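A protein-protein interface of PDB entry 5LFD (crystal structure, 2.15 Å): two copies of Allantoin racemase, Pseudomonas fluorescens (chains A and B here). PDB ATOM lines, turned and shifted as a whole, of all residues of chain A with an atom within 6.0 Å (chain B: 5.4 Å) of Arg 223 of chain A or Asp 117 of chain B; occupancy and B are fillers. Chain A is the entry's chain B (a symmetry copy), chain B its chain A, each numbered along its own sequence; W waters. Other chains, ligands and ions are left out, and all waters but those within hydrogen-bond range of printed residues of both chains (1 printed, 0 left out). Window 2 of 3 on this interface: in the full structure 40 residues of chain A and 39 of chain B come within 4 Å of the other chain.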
ATOM      1  N   SER A 220       1.317  10.327 -27.308  1.00  0.00           N
ATOM      2  CA  SER A 220       2.248  11.204 -26.589  1.00  0.00           C
ATOM      3  C   SER A 220       2.812  10.515 -25.336  1.00  0.00           C
ATOM      4  O   SER A 220       2.055   9.933 -24.562  1.00  0.00           O
ATOM      5  CB  SER A 220       1.508  12.428 -26.116  1.00  0.00           C
ATOM      6  OG  SER A 220       2.384  13.185 -25.342  1.00  0.00           O
ATOM      7  N   LYS A 221       4.132  10.577 -25.135  1.00  0.00           N
ATOM      8  CA  LYS A 221       4.739   9.890 -24.000  1.00  0.00           C
ATOM      9  C   LYS A 221       5.138  10.926 -22.920  1.00  0.00           C
ATOM     10  O   LYS A 221       5.923  10.624 -22.025  1.00  0.00           O
ATOM     11  CB  LYS A 221       5.990   9.063 -24.435  1.00  0.00           C
ATOM     12  CG  LYS A 221       5.774   8.065 -25.572  1.00  0.00           C
ATOM     13  CD  LYS A 221       4.654   7.030 -25.364  1.00  0.00           C
ATOM     14  CE  LYS A 221       4.974   6.014 -24.291  1.00  0.00           C
ATOM     15  NZ  LYS A 221       3.939   4.926 -24.298  1.00  0.00           N
ATOM     16  N   ILE A 222       4.592  12.128 -23.019  1.00  0.00           N
ATOM     17  CA  ILE A 222       5.017  13.272 -22.203  1.00  0.00           C
ATOM     18  C   ILE A 222       4.546  13.194 -20.751  1.00  0.00           C
ATOM     19  O   ILE A 222       5.193  13.693 -19.820  1.00  0.00           O
ATOM     20  CB  ILE A 222       4.634  14.656 -22.877  1.00  0.00           C
ATOM     21  CG1 ILE A 222       5.483  15.818 -22.307  1.00  0.00           C
ATOM     22  CG2 ILE A 222       3.139  15.000 -22.746  1.00  0.00           C
ATOM     23  CD1 ILE A 222       6.937  15.677 -22.676  1.00  0.00           C
ATOM     24  N   ARG A 223       3.405  12.573 -20.523  1.00  0.00           N
ATOM     25  CA  ARG A 223       2.891  12.668 -19.173  1.00  0.00           C
ATOM     26  C   ARG A 223       2.090  11.474 -18.831  1.00  0.00           C
ATOM     27  O   ARG A 223       2.619  10.508 -18.290  1.00  0.00           O
ATOM     28  CB  ARG A 223       2.088  13.988 -18.980  1.00  0.00           C
ATOM     29  CG  ARG A 223       1.567  14.221 -17.552  1.00  0.00           C
ATOM     30  CD  ARG A 223       0.485  15.315 -17.491  1.00  0.00           C
ATOM     31  NE  ARG A 223       0.270  15.718 -16.091  1.00  0.00           N
ATOM     32  CZ  ARG A 223      -0.821  16.347 -15.634  1.00  0.00           C
ATOM     33  NH1 ARG A 223      -1.829  16.621 -16.468  1.00  0.00           N
ATOM     34  NH2 ARG A 223      -0.908  16.705 -14.342  1.00  0.00           N
ATOM     35  N   THR A 224       0.798  11.535 -19.112  1.00  0.00           N
ATOM     36  CA  THR A 224      -0.119  10.498 -18.667  1.00  0.00           C
ATOM     37  C   THR A 224       0.269   9.107 -19.218  1.00  0.00           C
ATOM     38  O   THR A 224       0.115   8.110 -18.506  1.00  0.00           O
ATOM     39  CB  THR A 224      -1.537  10.769 -19.156  1.00  0.00           C
ATOM     40  OG1 THR A 224      -1.879  12.118 -18.834  1.00  0.00           O
ATOM     41  CG2 THR A 224      -2.564   9.769 -18.483  1.00  0.00           C
ATOM     42  N   TYR A 225       0.776   9.056 -20.457  1.00  0.00           N
ATOM     43  CA  TYR A 225       1.057   7.777 -21.106  1.00  0.00           C
ATOM     44  C   TYR A 225       2.548   7.583 -21.229  1.00  0.00           C
ATOM     45  O   TYR A 225       3.002   6.796 -22.061  1.00  0.00           O
ATOM     46  CB  TYR A 225       0.345   7.675 -22.462  1.00  0.00           C
ATOM     47  CG  TYR A 225      -1.126   7.876 -22.316  1.00  0.00           C
ATOM     48  CD1 TYR A 225      -1.902   6.989 -21.547  1.00  0.00           C
ATOM     49  CD2 TYR A 225      -1.745   8.964 -22.862  1.00  0.00           C
ATOM     50  CE1 TYR A 225      -3.262   7.184 -21.365  1.00  0.00           C
ATOM     51  CE2 TYR A 225      -3.119   9.142 -22.703  1.00  0.00           C
ATOM     52  CZ  TYR A 225      -3.861   8.253 -21.954  1.00  0.00           C
ATOM     53  OH  TYR A 225      -5.201   8.454 -21.784  1.00  0.00           O
ATOM     54  N   ALA A 226       3.313   8.280 -20.406  1.00  0.00           N
ATOM     55  CA  ALA A 226       4.728   7.944 -20.255  1.00  0.00           C
ATOM     56  C   ALA A 226       4.929   6.414 -20.114  1.00  0.00           C
ATOM     57  O   ALA A 226       4.087   5.696 -19.509  1.00  0.00           O
ATOM     58  CB  ALA A 226       5.276   8.635 -19.021  1.00  0.00           C
ATOM     59  N   THR B 115       1.316  11.938  -4.867  1.00  0.00           N
ATOM     60  CA  THR B 115       2.765  11.849  -5.041  1.00  0.00           C
ATOM     61  C   THR B 115       3.207  12.311  -6.441  1.00  0.00           C
ATOM     62  O   THR B 115       3.740  13.424  -6.624  1.00  0.00           O
ATOM     63  CB  THR B 115       3.235  10.395  -4.813  1.00  0.00           C
ATOM     64  OG1 THR B 115       2.479   9.514  -5.658  1.00  0.00           O
ATOM     65  CG2 THR B 115       2.970   9.982  -3.396  1.00  0.00           C
ATOM     66  N   LEU B 116       2.955  11.475  -7.447  1.00  0.00           N
ATOM     67  CA  LEU B 116       3.488  11.725  -8.777  1.00  0.00           C
ATOM     68  C   LEU B 116       2.571  12.510  -9.723  1.00  0.00           C
ATOM     69  O   LEU B 116       1.362  12.279  -9.791  1.00  0.00           O
ATOM     70  CB  LEU B 116       3.896  10.392  -9.411  1.00  0.00           C
ATOM     71  CG  LEU B 116       5.195   9.755  -8.863  1.00  0.00           C
ATOM     72  CD1 LEU B 116       5.516   8.500  -9.669  1.00  0.00           C
ATOM     73  CD2 LEU B 116       6.363  10.741  -8.950  1.00  0.00           C
ATOM     74  N   ASP B 117       3.167  13.437 -10.453  1.00  0.00           N
ATOM     75  CA  ASP B 117       2.441  14.186 -11.443  1.00  0.00           C
ATOM     76  C   ASP B 117       1.612  13.283 -12.383  1.00  0.00           C
ATOM     77  O   ASP B 117       0.455  13.606 -12.738  1.00  0.00           O
ATOM     78  CB  ASP B 117       3.394  15.069 -12.226  1.00  0.00           C
ATOM     79  CG  ASP B 117       2.676  15.896 -13.253  1.00  0.00           C
ATOM     80  OD1 ASP B 117       1.972  16.820 -12.829  1.00  0.00           O
ATOM     81  OD2 ASP B 117       2.769  15.603 -14.471  1.00  0.00           O
ATOM     82  N   ARG B 118       2.167  12.135 -12.774  1.00  0.00           N
ATOM     83  CA  ARG B 118       1.461  11.288 -13.762  1.00  0.00           C
ATOM     84  C   ARG B 118       0.227  10.602 -13.186  1.00  0.00           C
ATOM     85  O   ARG B 118      -0.614  10.147 -13.962  1.00  0.00           O
ATOM     86  CB  ARG B 118       2.381  10.256 -14.453  1.00  0.00           C
ATOM     87  CG  ARG B 118       2.727   9.065 -13.556  1.00  0.00           C
ATOM     88  CD  ARG B 118       3.639   8.100 -14.299  1.00  0.00           C
ATOM     89  NE  ARG B 118       2.936   7.536 -15.432  1.00  0.00           N
ATOM     90  CZ  ARG B 118       3.486   6.811 -16.396  1.00  0.00           C
ATOM     91  NH1 ARG B 118       4.789   6.527 -16.367  1.00  0.00           N
ATOM     92  NH2 ARG B 118       2.702   6.374 -17.391  1.00  0.00           N
ATOM     93  N   THR B 119       0.078  10.546 -11.864  1.00  0.00           N
ATOM     94  CA  THR B 119      -1.156  10.019 -11.281  1.00  0.00           C
ATOM     95  C   THR B 119      -2.273  11.056 -11.179  1.00  0.00           C
ATOM     96  O   THR B 119      -3.438  10.690 -11.003  1.00  0.00           O
ATOM     97  CB  THR B 119      -0.939   9.438  -9.895  1.00  0.00           C
ATOM     98  OG1 THR B 119      -0.878  10.512  -8.951  1.00  0.00           O
ATOM     99  CG2 THR B 119       0.406   8.615  -9.889  1.00  0.00           C
ATOM    100  N   VAL B 120      -1.908  12.340 -11.255  1.00  0.00           N
ATOM    101  CA  VAL B 120      -2.900  13.436 -11.199  1.00  0.00           C
ATOM    102  C   VAL B 120      -4.119  13.220 -12.112  1.00  0.00           C
ATOM    103  O   VAL B 120      -5.227  13.242 -11.637  1.00  0.00           O
ATOM    104  CB  VAL B 120      -2.272  14.794 -11.496  1.00  0.00           C
ATOM    105  CG1 VAL B 120      -3.351  15.878 -11.764  1.00  0.00           C
ATOM    106  CG2 VAL B 120      -1.276  15.154 -10.405  1.00  0.00           C
ATOM    107  N   PRO B 121      -3.910  12.979 -13.432  1.00  0.00           N
ATOM    108  CA  PRO B 121      -5.084  12.798 -14.269  1.00  0.00           C
ATOM    109  C   PRO B 121      -5.852  11.496 -14.053  1.00  0.00           C
ATOM    110  O   PRO B 121      -7.060  11.443 -14.353  1.00  0.00           O
ATOM    111  CB  PRO B 121      -4.517  12.865 -15.696  1.00  0.00           C
ATOM    112  CG  PRO B 121      -3.103  12.491 -15.542  1.00  0.00           C
ATOM    113  CD  PRO B 121      -2.665  12.994 -14.217  1.00  0.00           C
ATOM    114  N   ALA B 141       0.368  17.347  -7.383  1.00  0.00           N
ATOM    115  CA  ALA B 141       1.347  16.309  -7.072  1.00  0.00           C
ATOM    116  C   ALA B 141       2.451  16.907  -6.202  1.00  0.00           C
ATOM    117  O   ALA B 141       3.008  17.956  -6.521  1.00  0.00           O
ATOM    118  CB  ALA B 141       1.939  15.712  -8.329  1.00  0.00           C
ATOM    119  N   GLY B 143       5.268  15.573  -6.047  1.00  0.00           N
ATOM    120  CA  GLY B 143       6.518  15.217  -6.723  1.00  0.00           C
ATOM    121  C   GLY B 143       7.335  14.091  -6.064  1.00  0.00           C
ATOM    122  O   GLY B 143       8.321  13.613  -6.648  1.00  0.00           O
HETATM  123  O   HOH W   1       0.228   7.996 -15.668  1.00  0.00           O
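No position is printed for both chains.
Of the 7 printed residues of chain A, 3 touch a printed residue of chain B. Hydrophobic or aromatic side chains of chain A within 4 Å of the printed part of chain B: Ala 226. Of the 9 printed residues of chain B, 4 touch a printed residue of chain A. Hydrophobic or aromatic side chains of chain B within 4 Å of the printed part of chain A: Val 120 and Pro 121. Among the printed residues, 6 pairs touch across the chains. Among the printed residues, Asp or Glu carboxylates within 4 Å of a Lys or Arg side-chain nitrogen of the other chain: Arg 223 of chain A with Asp 117 of chain B (3.0 Å).
The guanidinium group of Arg 223 of chain A is in salt-bridge range of the side-chain carboxylate of Asp 117 of chain B (3.0 Å). The guanidinium group of Arg 118 of chain B sits at hydrogen-bond distance from the backbone carbonyl oxygen of Thr 224 of chain A, 3.3 Å away. The guanidinium group of Arg 118 of chain B sits at hydrogen-bond distance from the backbone carbonyl oxygen of Ala 226 of chain A (2.6 Å).
Ile 222 of chain A touches none of the printed residues of chain B. Arg 223 of chain A touches just these residues of chain B: Asp 117 (3.0 Å), Arg 118 (3.9 Å) and Val 120 (3.6 Å). Of the printed residues of chain B, Thr 224 of chain A touches Arg 118 and Pro 121. Of the printed residues of chain B, Ala 226 of chain A touches Arg 118. Of chain A, only Arg 223 (3.0 Å) comes within 4 Å of Asp 117 of chain B. Printed residues of chain A within 4 Å of Val 120 of chain B: Arg 223. Printed residues of chain A within 4 Å of Pro 121 of chain B: Thr 224. Ala 141 of chain B touches none of the printed residues of chain A.
Among the printed residues, merely in contact across the chains: Thr 224 of chain A with Pro 121 of chain B (3.5 Å), Arg 223 of chain A with Val 120 of chain B (3.6 Å) and Arg 223 of chain A with Arg 118 of chain B (3.9 Å).
Water W1 bridges the guanidinium group of Arg 118 of chain B (2.8 Å) and the backbone carbonyl oxygen of Thr 224 of chain A (2.8 Å).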
